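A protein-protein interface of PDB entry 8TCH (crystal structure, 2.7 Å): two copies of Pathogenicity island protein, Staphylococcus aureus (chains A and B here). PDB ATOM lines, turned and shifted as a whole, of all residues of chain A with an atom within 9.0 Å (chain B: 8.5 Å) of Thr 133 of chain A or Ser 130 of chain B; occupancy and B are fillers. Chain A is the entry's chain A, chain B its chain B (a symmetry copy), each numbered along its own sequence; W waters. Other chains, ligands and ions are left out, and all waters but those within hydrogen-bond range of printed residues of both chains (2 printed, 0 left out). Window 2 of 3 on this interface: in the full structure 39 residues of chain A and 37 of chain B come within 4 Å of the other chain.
The side-chain carboxylate of Asp 113 of chain A is in hydrogen-bond range of the backbone NH of Arg 115 of chain A. The side-chain hydroxyl (OG1) of Thr 131 of chain B lies within hydrogen-bond range of the backbone NH (N) of Thr 128 of chain B. The side-chain hydroxyl (OG1) of Thr 128 of chain B sits close to the backbone NH (N) of Ser 130 of chain B (3.1 Å). The side-chain amino group (NZ) of Lys 134 of chain B sits at hydrogen-bond distance from the backbone carbonyl oxygen (O) of Ser 130 of chain B (3.4 Å).
CD1 of Leu 118 of chain B touches O of Ser 112 of chain A, at 3.8 Å. Val 127 of chain B touches Ser 112 of chain A (O to CB, 3.6 Å). Thr 128 of chain B touches Ser 112 of chain A (CA to O, 3.3 Å). Asp 113 of chain A touches Leu 118 of chain B. Ser 129 of chain B touches Asp 113 of chain A. CG2 of Thr 133 of chain A touches OG of Ser 130 of chain B, at 3.7 Å. Val 136 of chain A touches Thr 128 of chain B (CG1 to CB, 3.99 Å). ND2 of Asn 140 of chain A touches CE1 of Phe 69 of chain B, at 3.96 Å. Thr 128 of chain B touches Asn 140 of chain A (CG2 to ND2, 3.8 Å).
Water W1 lies within hydrogen-bond range of the side-chain carboxylate of Asp 137 of chain A (2.6 Å), the side-chain amide nitrogen of Asn 140 of chain A (3.2 Å) and the side-chain hydroxyl of Thr 128 of chain B (3.3 Å). Water W2 lies within hydrogen-bond range of the side-chain amide nitrogen (ND2) of Asn 140 of chain A (3.0 Å), the side-chain hydroxyl (OG1) of Thr 131 of chain B (3.2 Å) and the backbone carbonyl oxygen (O) of Ile 70 of chain B (3.3 Å).
Of the printed residues of chain A, Leu 118 of chain B touches Ser 112 and Asp 113. Printed residues of chain B within 4 Å of Asp 137 of chain A: Ser 130 (2.7 Å). Of the printed residues of chain B, Asn 140 of chain A touches Phe 69 and Thr 128. Printed residues of chain B within 4 Å of Ser 114 of chain A: Ser 129 (3.3 Å). Ser 132 of chain B touches none of the printed residues of chain A. Ile 139 of chain A touches none of the printed residues of chain B. The nearest residue of chain A that does not touch Ser 130 of chain B is Val 136 of chain A (4.4 Å).
Printed residues of chain B that touch a printed residue of chain A: Phe 69, Leu 118, Val 127, Thr 128, Ser 129 and Ser 130. Hydrophobic or aromatic side chains of chain B within 4 Å of the printed part of chain A: Phe 69 and Leu 118. Printed residues of chain A that touch a printed residue of chain B: Ser 112, Asp 113, Ser 114, Thr 133, Val 136, Asp 137 and Asn 140. Hydrophobic or aromatic side chains of chain A that line the printed part of chain B: Val 136. Along chain A the printed residues that touch a printed residue of chain B span positions 112 to 140. Among the printed residues, 12 pairs touch across the chains.
N of Ser 129 of chain B sits at hydrogen-bond distance from O of Ser 112 of chain A (3.1 Å). N of Ser 114 of chain A is in hydrogen-bond range of OG of Ser 129 of chain B. OD1 of Asp 137 of chain A is in hydrogen-bond range of OG of Ser 130 of chain B.
Ser 114 of chain A touches Ser 129 of chain B, but with the chains exchanged Ser 129 of chain A does not touch Ser 114 of chain B (17.3 Å). Thr 133 of chain A touches Ser 130 of chain B, but with the chains exchanged Ser 130 of chain A does not touch Thr 133 of chain B (17.2 Å).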
ATOM      1  N   TYR A  41     -13.491 -27.553  41.341  1.00  0.00           N
ATOM      2  CA  TYR A  41     -12.722 -26.333  41.515  1.00  0.00           C
ATOM      3  C   TYR A  41     -12.425 -26.093  42.989  1.00  0.00           C
ATOM      4  O   TYR A  41     -13.201 -26.466  43.874  1.00  0.00           O
ATOM      5  CB  TYR A  41     -13.478 -25.144  40.919  1.00  0.00           C
ATOM      6  CG  TYR A  41     -13.748 -25.330  39.444  1.00  0.00           C
ATOM      7  CD1 TYR A  41     -12.803 -24.966  38.493  1.00  0.00           C
ATOM      8  CD2 TYR A  41     -14.935 -25.902  39.002  1.00  0.00           C
ATOM      9  CE1 TYR A  41     -13.039 -25.147  37.144  1.00  0.00           C
ATOM     10  CE2 TYR A  41     -15.180 -26.088  37.653  1.00  0.00           C
ATOM     11  CZ  TYR A  41     -14.228 -25.709  36.729  1.00  0.00           C
ATOM     12  OH  TYR A  41     -14.462 -25.886  35.383  1.00  0.00           O
ATOM     13  N   GLN A  54      -8.112 -25.373  39.340  1.00  0.00           N
ATOM     14  CA  GLN A  54      -8.817 -26.552  38.858  1.00  0.00           C
ATOM     15  C   GLN A  54      -8.258 -27.786  39.552  1.00  0.00           C
ATOM     16  O   GLN A  54      -7.047 -27.897  39.768  1.00  0.00           O
ATOM     17  CB  GLN A  54      -8.681 -26.700  37.343  1.00  0.00           C
ATOM     18  CG  GLN A  54      -9.651 -27.713  36.752  1.00  0.00           C
ATOM     19  CD  GLN A  54      -9.325 -28.082  35.318  1.00  0.00           C
ATOM     20  OE1 GLN A  54      -8.257 -27.751  34.803  1.00  0.00           O
ATOM     21  NE2 GLN A  54     -10.247 -28.782  34.666  1.00  0.00           N
ATOM     22  N   ILE A  70      -6.201 -21.124  37.668  1.00  0.00           N
ATOM     23  CA  ILE A  70      -7.071 -20.594  36.628  1.00  0.00           C
ATOM     24  C   ILE A  70      -7.052 -19.071  36.615  1.00  0.00           C
ATOM     25  O   ILE A  70      -6.824 -18.453  35.574  1.00  0.00           O
ATOM     26  CB  ILE A  70      -8.512 -21.124  36.787  1.00  0.00           C
ATOM     27  CG1 ILE A  70      -8.549 -22.639  36.592  1.00  0.00           C
ATOM     28  CG2 ILE A  70      -9.442 -20.424  35.810  1.00  0.00           C
ATOM     29  CD1 ILE A  70      -9.943 -23.209  36.601  1.00  0.00           C
ATOM     30  N   ILE A 111     -18.515 -14.463  27.073  1.00  0.00           N
ATOM     31  CA  ILE A 111     -18.444 -15.340  28.229  1.00  0.00           C
ATOM     32  C   ILE A 111     -18.239 -16.791  27.811  1.00  0.00           C
ATOM     33  O   ILE A 111     -17.655 -17.575  28.566  1.00  0.00           O
ATOM     34  CB  ILE A 111     -19.715 -15.174  29.079  1.00  0.00           C
ATOM     35  CG1 ILE A 111     -19.570 -13.954  29.988  1.00  0.00           C
ATOM     36  CG2 ILE A 111     -19.998 -16.435  29.872  1.00  0.00           C
ATOM     37  CD1 ILE A 111     -20.687 -13.794  30.992  1.00  0.00           C
ATOM     38  N   SER A 112     -18.692 -17.177  26.621  1.00  0.00           N
ATOM     39  CA  SER A 112     -18.686 -18.581  26.230  1.00  0.00           C
ATOM     40  C   SER A 112     -17.690 -18.912  25.123  1.00  0.00           C
ATOM     41  O   SER A 112     -17.702 -20.039  24.616  1.00  0.00           O
ATOM     42  CB  SER A 112     -20.095 -19.001  25.801  1.00  0.00           C
ATOM     43  OG  SER A 112     -20.447 -18.365  24.588  1.00  0.00           O
ATOM     44  N   ASP A 113     -16.826 -17.977  24.738  1.00  0.00           N
ATOM     45  CA  ASP A 113     -15.845 -18.205  23.678  1.00  0.00           C
ATOM     46  C   ASP A 113     -14.489 -17.733  24.179  1.00  0.00           C
ATOM     47  O   ASP A 113     -14.299 -16.539  24.433  1.00  0.00           O
ATOM     48  CB  ASP A 113     -16.253 -17.477  22.393  1.00  0.00           C
ATOM     49  CG  ASP A 113     -15.281 -17.705  21.243  1.00  0.00           C
ATOM     50  OD1 ASP A 113     -14.184 -18.259  21.466  1.00  0.00           O
ATOM     51  OD2 ASP A 113     -15.627 -17.334  20.101  1.00  0.00           O
ATOM     52  N   SER A 114     -13.548 -18.672  24.310  1.00  0.00           N
ATOM     53  CA  SER A 114     -12.270 -18.367  24.944  1.00  0.00           C
ATOM     54  C   SER A 114     -11.562 -17.205  24.259  1.00  0.00           C
ATOM     55  O   SER A 114     -11.075 -16.282  24.923  1.00  0.00           O
ATOM     56  CB  SER A 114     -11.385 -19.613  24.932  1.00  0.00           C
ATOM     57  OG  SER A 114     -11.528 -20.312  23.705  1.00  0.00           O
ATOM     58  N   ARG A 115     -11.493 -17.233  22.928  1.00  0.00           N
ATOM     59  CA  ARG A 115     -10.764 -16.196  22.202  1.00  0.00           C
ATOM     60  C   ARG A 115     -11.384 -14.827  22.437  1.00  0.00           C
ATOM     61  O   ARG A 115     -10.671 -13.817  22.434  1.00  0.00           O
ATOM     62  CB  ARG A 115     -10.689 -16.561  20.720  1.00  0.00           C
ATOM     63  CG  ARG A 115     -10.058 -17.947  20.544  1.00  0.00           C
ATOM     64  CD  ARG A 115      -8.527 -17.931  20.699  1.00  0.00           C
ATOM     65  NE  ARG A 115      -7.842 -17.342  19.555  1.00  0.00           N
ATOM     66  CZ  ARG A 115      -6.979 -17.998  18.777  1.00  0.00           C
ATOM     67  NH1 ARG A 115      -6.662 -19.263  19.027  1.00  0.00           N
ATOM     68  NH2 ARG A 115      -6.422 -17.381  17.750  1.00  0.00           N
ATOM     69  N   LEU A 117     -13.509 -14.161  25.302  1.00  0.00           N
ATOM     70  CA  LEU A 117     -13.316 -13.936  26.733  1.00  0.00           C
ATOM     71  C   LEU A 117     -11.975 -13.270  27.003  1.00  0.00           C
ATOM     72  O   LEU A 117     -11.862 -12.394  27.869  1.00  0.00           O
ATOM     73  CB  LEU A 117     -13.394 -15.256  27.498  1.00  0.00           C
ATOM     74  CG  LEU A 117     -13.343 -15.112  29.022  1.00  0.00           C
ATOM     75  CD1 LEU A 117     -14.609 -14.439  29.533  1.00  0.00           C
ATOM     76  CD2 LEU A 117     -13.135 -16.455  29.706  1.00  0.00           C
ATOM     77  N   LEU A 118     -10.942 -13.687  26.273  1.00  0.00           N
ATOM     78  CA  LEU A 118      -9.610 -13.121  26.436  1.00  0.00           C
ATOM     79  C   LEU A 118      -9.593 -11.607  26.268  1.00  0.00           C
ATOM     80  O   LEU A 118      -8.671 -10.955  26.764  1.00  0.00           O
ATOM     81  CB  LEU A 118      -8.670 -13.781  25.428  1.00  0.00           C
ATOM     82  CG  LEU A 118      -7.168 -13.584  25.582  1.00  0.00           C
ATOM     83  CD1 LEU A 118      -6.723 -13.910  26.993  1.00  0.00           C
ATOM     84  CD2 LEU A 118      -6.452 -14.474  24.575  1.00  0.00           C
ATOM     85  N   VAL A 127      -7.042 -13.270  32.899  1.00  0.00           N
ATOM     86  CA  VAL A 127      -7.207 -14.347  31.932  1.00  0.00           C
ATOM     87  C   VAL A 127      -6.092 -14.217  30.906  1.00  0.00           C
ATOM     88  O   VAL A 127      -5.559 -13.129  30.674  1.00  0.00           O
ATOM     89  CB  VAL A 127      -8.603 -14.307  31.268  1.00  0.00           C
ATOM     90  CG1 VAL A 127      -8.748 -13.077  30.388  1.00  0.00           C
ATOM     91  CG2 VAL A 127      -8.851 -15.575  30.460  1.00  0.00           C
ATOM     92  N   THR A 128      -5.727 -15.344  30.305  1.00  0.00           N
ATOM     93  CA  THR A 128      -4.692 -15.377  29.287  1.00  0.00           C
ATOM     94  C   THR A 128      -5.094 -16.380  28.217  1.00  0.00           C
ATOM     95  O   THR A 128      -6.051 -17.144  28.380  1.00  0.00           O
ATOM     96  CB  THR A 128      -3.328 -15.762  29.873  1.00  0.00           C
ATOM     97  OG1 THR A 128      -3.359 -17.140  30.270  1.00  0.00           O
ATOM     98  CG2 THR A 128      -2.996 -14.900  31.077  1.00  0.00           C
ATOM     99  N   SER A 129      -4.343 -16.390  27.116  1.00  0.00           N
ATOM    100  CA  SER A 129      -4.558 -17.410  26.101  1.00  0.00           C
ATOM    101  C   SER A 129      -4.337 -18.812  26.653  1.00  0.00           C
ATOM    102  O   SER A 129      -4.866 -19.779  26.093  1.00  0.00           O
ATOM    103  CB  SER A 129      -3.637 -17.159  24.907  1.00  0.00           C
ATOM    104  OG  SER A 129      -2.312 -16.895  25.334  1.00  0.00           O
ATOM    105  N   SER A 130      -3.584 -18.941  27.749  1.00  0.00           N
ATOM    106  CA  SER A 130      -3.356 -20.247  28.358  1.00  0.00           C
ATOM    107  C   SER A 130      -4.529 -20.675  29.232  1.00  0.00           C
ATOM    108  O   SER A 130      -4.914 -21.850  29.221  1.00  0.00           O
ATOM    109  CB  SER A 130      -2.069 -20.216  29.183  1.00  0.00           C
ATOM    110  OG  SER A 130      -0.982 -19.753  28.404  1.00  0.00           O
ATOM    111  N   THR A 131      -5.118 -19.743  29.980  1.00  0.00           N
ATOM    112  CA  THR A 131      -6.172 -20.068  30.932  1.00  0.00           C
ATOM    113  C   THR A 131      -7.571 -19.753  30.415  1.00  0.00           C
ATOM    114  O   THR A 131      -8.546 -19.949  31.149  1.00  0.00           O
ATOM    115  CB  THR A 131      -5.948 -19.316  32.252  1.00  0.00           C
ATOM    116  OG1 THR A 131      -5.915 -17.904  32.003  1.00  0.00           O
ATOM    117  CG2 THR A 131      -4.645 -19.740  32.905  1.00  0.00           C
ATOM    118  N   SER A 132      -7.699 -19.275  29.174  1.00  0.00           N
ATOM    119  CA  SER A 132      -9.002 -18.856  28.668  1.00  0.00           C
ATOM    120  C   SER A 132     -10.004 -20.007  28.665  1.00  0.00           C
ATOM    121  O   SER A 132     -11.168 -19.821  29.037  1.00  0.00           O
ATOM    122  CB  SER A 132      -8.849 -18.288  27.258  1.00  0.00           C
ATOM    123  OG  SER A 132      -8.347 -19.276  26.376  1.00  0.00           O
ATOM    124  N   THR A 133      -9.578 -21.200  28.244  1.00  0.00           N
ATOM    125  CA  THR A 133     -10.499 -22.331  28.161  1.00  0.00           C
ATOM    126  C   THR A 133     -10.959 -22.773  29.548  1.00  0.00           C
ATOM    127  O   THR A 133     -12.150 -23.031  29.764  1.00  0.00           O
ATOM    128  CB  THR A 133      -9.835 -23.491  27.413  1.00  0.00           C
ATOM    129  OG1 THR A 133      -9.692 -23.143  26.029  1.00  0.00           O
ATOM    130  CG2 THR A 133     -10.658 -24.770  27.520  1.00  0.00           C
ATOM    131  N   LYS A 134     -10.020 -22.916  30.487  1.00  0.00           N
ATOM    132  CA  LYS A 134     -10.391 -23.315  31.841  1.00  0.00           C
ATOM    133  C   LYS A 134     -11.330 -22.297  32.471  1.00  0.00           C
ATOM    134  O   LYS A 134     -12.248 -22.671  33.209  1.00  0.00           O
ATOM    135  CB  LYS A 134      -9.130 -23.498  32.690  1.00  0.00           C
ATOM    136  CG  LYS A 134      -8.286 -24.701  32.262  1.00  0.00           C
ATOM    137  CD  LYS A 134      -7.022 -24.879  33.101  1.00  0.00           C
ATOM    138  CE  LYS A 134      -6.030 -23.740  32.897  1.00  0.00           C
ATOM    139  NZ  LYS A 134      -5.324 -23.832  31.587  1.00  0.00           N
ATOM    140  N   LEU A 135     -11.147 -21.012  32.158  1.00  0.00           N
ATOM    141  CA  LEU A 135     -12.027 -19.985  32.707  1.00  0.00           C
ATOM    142  C   LEU A 135     -13.396 -20.024  32.039  1.00  0.00           C
ATOM    143  O   LEU A 135     -14.419 -19.804  32.698  1.00  0.00           O
ATOM    144  CB  LEU A 135     -11.378 -18.611  32.551  1.00  0.00           C
ATOM    145  CG  LEU A 135     -12.079 -17.433  33.227  1.00  0.00           C
ATOM    146  CD1 LEU A 135     -12.370 -17.713  34.693  1.00  0.00           C
ATOM    147  CD2 LEU A 135     -11.229 -16.173  33.089  1.00  0.00           C
ATOM    148  N   VAL A 136     -13.443 -20.318  30.738  1.00  0.00           N
ATOM    149  CA  VAL A 136     -14.726 -20.508  30.066  1.00  0.00           C
ATOM    150  C   VAL A 136     -15.490 -21.661  30.707  1.00  0.00           C
ATOM    151  O   VAL A 136     -16.693 -21.560  30.988  1.00  0.00           O
ATOM    152  CB  VAL A 136     -14.508 -20.746  28.561  1.00  0.00           C
ATOM    153  CG1 VAL A 136     -15.783 -21.261  27.910  1.00  0.00           C
ATOM    154  CG2 VAL A 136     -14.041 -19.460  27.885  1.00  0.00           C
ATOM    155  N   ASP A 137     -14.800 -22.775  30.952  1.00  0.00           N
ATOM    156  CA  ASP A 137     -15.449 -23.935  31.549  1.00  0.00           C
ATOM    157  C   ASP A 137     -15.918 -23.634  32.968  1.00  0.00           C
ATOM    158  O   ASP A 137     -17.021 -24.036  33.368  1.00  0.00           O
ATOM    159  CB  ASP A 137     -14.496 -25.129  31.535  1.00  0.00           C
ATOM    160  CG  ASP A 137     -14.192 -25.616  30.132  1.00  0.00           C
ATOM    161  OD1 ASP A 137     -15.030 -25.393  29.230  1.00  0.00           O
ATOM    162  OD2 ASP A 137     -13.120 -26.220  29.927  1.00  0.00           O
ATOM    163  N   TYR A 138     -15.094 -22.929  33.748  1.00  0.00           N
ATOM    164  CA  TYR A 138     -15.522 -22.557  35.088  1.00  0.00           C
ATOM    165  C   TYR A 138     -16.755 -21.669  35.037  1.00  0.00           C
ATOM    166  O   TYR A 138     -17.672 -21.824  35.847  1.00  0.00           O
ATOM    167  CB  TYR A 138     -14.416 -21.835  35.845  1.00  0.00           C
ATOM    168  CG  TYR A 138     -14.917 -21.320  37.173  1.00  0.00           C
ATOM    169  CD1 TYR A 138     -15.041 -22.173  38.261  1.00  0.00           C
ATOM    170  CD2 TYR A 138     -15.302 -19.998  37.333  1.00  0.00           C
ATOM    171  CE1 TYR A 138     -15.511 -21.718  39.475  1.00  0.00           C
ATOM    172  CE2 TYR A 138     -15.775 -19.534  38.545  1.00  0.00           C
ATOM    173  CZ  TYR A 138     -15.878 -20.398  39.610  1.00  0.00           C
ATOM    174  OH  TYR A 138     -16.347 -19.943  40.819  1.00  0.00           O
ATOM    175  N   ILE A 139     -16.768 -20.696  34.126  1.00  0.00           N
ATOM    176  CA  ILE A 139     -17.920 -19.813  33.990  1.00  0.00           C
ATOM    177  C   ILE A 139     -19.170 -20.625  33.674  1.00  0.00           C
ATOM    178  O   ILE A 139     -20.234 -20.413  34.265  1.00  0.00           O
ATOM    179  CB  ILE A 139     -17.642 -18.751  32.912  1.00  0.00           C
ATOM    180  CG1 ILE A 139     -16.738 -17.647  33.470  1.00  0.00           C
ATOM    181  CG2 ILE A 139     -18.940 -18.169  32.407  1.00  0.00           C
ATOM    182  CD1 ILE A 139     -16.137 -16.741  32.406  1.00  0.00           C
ATOM    183  N   ASN A 140     -19.063 -21.560  32.731  1.00  0.00           N
ATOM    184  CA  ASN A 140     -20.208 -22.396  32.380  1.00  0.00           C
ATOM    185  C   ASN A 140     -20.721 -23.162  33.598  1.00  0.00           C
ATOM    186  O   ASN A 140     -21.931 -23.207  33.869  1.00  0.00           O
ATOM    187  CB  ASN A 140     -19.811 -23.348  31.250  1.00  0.00           C
ATOM    188  CG  ASN A 140     -20.989 -24.107  30.677  1.00  0.00           C
ATOM    189  OD1 ASN A 140     -22.145 -23.750  30.896  1.00  0.00           O
ATOM    190  ND2 ASN A 140     -20.695 -25.160  29.926  1.00  0.00           N
ATOM    191  N   ALA A 141     -19.804 -23.759  34.365  1.00  0.00           N
ATOM    192  CA  ALA A 141     -20.219 -24.556  35.517  1.00  0.00           C
ATOM    193  C   ALA A 141     -20.843 -23.678  36.598  1.00  0.00           C
ATOM    194  O   ALA A 141     -21.907 -24.001  37.140  1.00  0.00           O
ATOM    195  CB  ALA A 141     -19.029 -25.338  36.070  1.00  0.00           C
ATOM    196  N   VAL B  68     -19.264 -36.886  30.495  1.00  0.00           N
ATOM    197  CA  VAL B  68     -18.699 -35.627  30.017  1.00  0.00           C
ATOM    198  C   VAL B  68     -19.866 -34.719  29.646  1.00  0.00           C
ATOM    199  O   VAL B  68     -20.615 -35.016  28.707  1.00  0.00           O
ATOM    200  CB  VAL B  68     -17.761 -35.832  28.819  1.00  0.00           C
ATOM    201  CG1 VAL B  68     -17.162 -34.505  28.374  1.00  0.00           C
ATOM    202  CG2 VAL B  68     -16.661 -36.824  29.171  1.00  0.00           C
ATOM    203  N   PHE B  69     -20.029 -33.623  30.387  1.00  0.00           N
ATOM    204  CA  PHE B  69     -21.151 -32.720  30.161  1.00  0.00           C
ATOM    205  C   PHE B  69     -21.063 -32.080  28.780  1.00  0.00           C
ATOM    206  O   PHE B  69     -19.996 -31.631  28.350  1.00  0.00           O
ATOM    207  CB  PHE B  69     -21.177 -31.631  31.238  1.00  0.00           C
ATOM    208  CG  PHE B  69     -22.199 -30.557  30.989  1.00  0.00           C
ATOM    209  CD1 PHE B  69     -21.901 -29.470  30.182  1.00  0.00           C
ATOM    210  CD2 PHE B  69     -23.454 -30.627  31.568  1.00  0.00           C
ATOM    211  CE1 PHE B  69     -22.837 -28.485  29.950  1.00  0.00           C
ATOM    212  CE2 PHE B  69     -24.392 -29.640  31.341  1.00  0.00           C
ATOM    213  CZ  PHE B  69     -24.082 -28.570  30.533  1.00  0.00           C
ATOM    214  N   ILE B  70     -22.201 -32.020  28.095  1.00  0.00           N
ATOM    215  CA  ILE B  70     -22.309 -31.364  26.799  1.00  0.00           C
ATOM    216  C   ILE B  70     -23.107 -30.067  26.899  1.00  0.00           C
ATOM    217  O   ILE B  70     -22.630 -29.004  26.498  1.00  0.00           O
ATOM    218  CB  ILE B  70     -22.926 -32.311  25.745  1.00  0.00           C
ATOM    219  CG1 ILE B  70     -22.009 -33.514  25.510  1.00  0.00           C
ATOM    220  CG2 ILE B  70     -23.174 -31.565  24.440  1.00  0.00           C
ATOM    221  CD1 ILE B  70     -22.469 -34.431  24.396  1.00  0.00           C
ATOM    222  N   SER B 114     -18.872 -26.294  14.299  1.00  0.00           N
ATOM    223  CA  SER B 114     -18.754 -25.886  15.695  1.00  0.00           C
ATOM    224  C   SER B 114     -18.568 -24.380  15.822  1.00  0.00           C
ATOM    225  O   SER B 114     -19.182 -23.738  16.687  1.00  0.00           O
ATOM    226  CB  SER B 114     -17.591 -26.633  16.347  1.00  0.00           C
ATOM    227  OG  SER B 114     -16.510 -26.751  15.442  1.00  0.00           O
ATOM    228  N   LEU B 118     -21.448 -22.204  17.771  1.00  0.00           N
ATOM    229  CA  LEU B 118     -21.140 -21.391  18.941  1.00  0.00           C
ATOM    230  C   LEU B 118     -21.842 -20.039  18.920  1.00  0.00           C
ATOM    231  O   LEU B 118     -22.022 -19.438  19.984  1.00  0.00           O
ATOM    232  CB  LEU B 118     -19.629 -21.176  19.046  1.00  0.00           C
ATOM    233  CG  LEU B 118     -19.128 -20.565  20.354  1.00  0.00           C
ATOM    234  CD1 LEU B 118     -19.655 -21.313  21.567  1.00  0.00           C
ATOM    235  CD2 LEU B 118     -17.608 -20.542  20.369  1.00  0.00           C
ATOM    236  N   VAL B 127     -23.880 -23.546  24.943  1.00  0.00           N
ATOM    237  CA  VAL B 127     -22.774 -24.085  24.160  1.00  0.00           C
ATOM    238  C   VAL B 127     -21.563 -23.200  24.413  1.00  0.00           C
ATOM    239  O   VAL B 127     -21.694 -22.021  24.751  1.00  0.00           O
ATOM    240  CB  VAL B 127     -23.140 -24.165  22.658  1.00  0.00           C
ATOM    241  CG1 VAL B 127     -23.262 -22.773  22.057  1.00  0.00           C
ATOM    242  CG2 VAL B 127     -22.132 -25.008  21.890  1.00  0.00           C
ATOM    243  N   THR B 128     -20.375 -23.784  24.267  1.00  0.00           N
ATOM    244  CA  THR B 128     -19.129 -23.060  24.461  1.00  0.00           C
ATOM    245  C   THR B 128     -18.126 -23.518  23.412  1.00  0.00           C
ATOM    246  O   THR B 128     -18.360 -24.480  22.677  1.00  0.00           O
ATOM    247  CB  THR B 128     -18.544 -23.284  25.862  1.00  0.00           C
ATOM    248  OG1 THR B 128     -18.081 -24.638  25.975  1.00  0.00           O
ATOM    249  CG2 THR B 128     -19.587 -23.026  26.934  1.00  0.00           C
ATOM    250  N   SER B 129     -16.996 -22.809  23.336  1.00  0.00           N
ATOM    251  CA  SER B 129     -15.904 -23.263  22.483  1.00  0.00           C
ATOM    252  C   SER B 129     -15.369 -24.619  22.929  1.00  0.00           C
ATOM    253  O   SER B 129     -14.742 -25.322  22.129  1.00  0.00           O
ATOM    254  CB  SER B 129     -14.778 -22.227  22.469  1.00  0.00           C
ATOM    255  OG  SER B 129     -14.466 -21.783  23.778  1.00  0.00           O
ATOM    256  N   SER B 130     -15.606 -24.998  24.189  1.00  0.00           N
ATOM    257  CA  SER B 130     -15.162 -26.294  24.687  1.00  0.00           C
ATOM    258  C   SER B 130     -16.113 -27.412  24.276  1.00  0.00           C
ATOM    259  O   SER B 130     -15.670 -28.523  23.958  1.00  0.00           O
ATOM    260  CB  SER B 130     -15.036 -26.252  26.213  1.00  0.00           C
ATOM    261  OG  SER B 130     -14.215 -25.176  26.629  1.00  0.00           O
ATOM    262  N   THR B 131     -17.417 -27.147  24.292  1.00  0.00           N
ATOM    263  CA  THR B 131     -18.412 -28.175  24.028  1.00  0.00           C
ATOM    264  C   THR B 131     -19.004 -28.108  22.627  1.00  0.00           C
ATOM    265  O   THR B 131     -19.871 -28.925  22.300  1.00  0.00           O
ATOM    266  CB  THR B 131     -19.545 -28.078  25.058  1.00  0.00           C
ATOM    267  OG1 THR B 131     -20.150 -26.780  24.985  1.00  0.00           O
ATOM    268  CG2 THR B 131     -19.010 -28.296  26.464  1.00  0.00           C
ATOM    269  N   SER B 132     -18.559 -27.173  21.786  1.00  0.00           N
ATOM    270  CA  SER B 132     -19.182 -27.006  20.476  1.00  0.00           C
ATOM    271  C   SER B 132     -19.083 -28.280  19.639  1.00  0.00           C
ATOM    272  O   SER B 132     -20.046 -28.661  18.962  1.00  0.00           O
ATOM    273  CB  SER B 132     -18.542 -25.830  19.740  1.00  0.00           C
ATOM    274  OG  SER B 132     -17.164 -26.068  19.521  1.00  0.00           O
ATOM    275  N   THR B 133     -17.929 -28.950  19.667  1.00  0.00           N
ATOM    276  CA  THR B 133     -17.742 -30.144  18.846  1.00  0.00           C
ATOM    277  C   THR B 133     -18.644 -31.285  19.307  1.00  0.00           C
ATOM    278  O   THR B 133     -19.302 -31.944  18.486  1.00  0.00           O
ATOM    279  CB  THR B 133     -16.274 -30.579  18.884  1.00  0.00           C
ATOM    280  OG1 THR B 133     -15.473 -29.633  18.163  1.00  0.00           O
ATOM    281  CG2 THR B 133     -16.098 -31.960  18.276  1.00  0.00           C
ATOM    282  N   LYS B 134     -18.673 -31.553  20.615  1.00  0.00           N
ATOM    283  CA  LYS B 134     -19.532 -32.617  21.122  1.00  0.00           C
ATOM    284  C   LYS B 134     -20.998 -32.330  20.835  1.00  0.00           C
ATOM    285  O   LYS B 134     -21.768 -33.258  20.565  1.00  0.00           O
ATOM    286  CB  LYS B 134     -19.305 -32.819  22.622  1.00  0.00           C
ATOM    287  CG  LYS B 134     -17.946 -33.426  22.958  1.00  0.00           C
ATOM    288  CD  LYS B 134     -17.759 -33.645  24.460  1.00  0.00           C
ATOM    289  CE  LYS B 134     -17.695 -32.341  25.245  1.00  0.00           C
ATOM    290  NZ  LYS B 134     -16.389 -31.642  25.085  1.00  0.00           N
ATOM    291  N   LEU B 135     -21.404 -31.058  20.862  1.00  0.00           N
ATOM    292  CA  LEU B 135     -22.799 -30.733  20.575  1.00  0.00           C
ATOM    293  C   LEU B 135     -23.100 -30.877  19.088  1.00  0.00           C
ATOM    294  O   LEU B 135     -24.194 -31.313  18.714  1.00  0.00           O
ATOM    295  CB  LEU B 135     -23.130 -29.324  21.060  1.00  0.00           C
ATOM    296  CG  LEU B 135     -24.603 -28.915  20.962  1.00  0.00           C
ATOM    297  CD1 LEU B 135     -25.514 -29.955  21.605  1.00  0.00           C
ATOM    298  CD2 LEU B 135     -24.824 -27.548  21.606  1.00  0.00           C
HETATM  299  O   HOH W   1     -17.618 -25.610  29.105  1.00  0.00           O
HETATM  300  O   HOH W   2     -22.087 -25.890  27.419  1.00  0.00           O
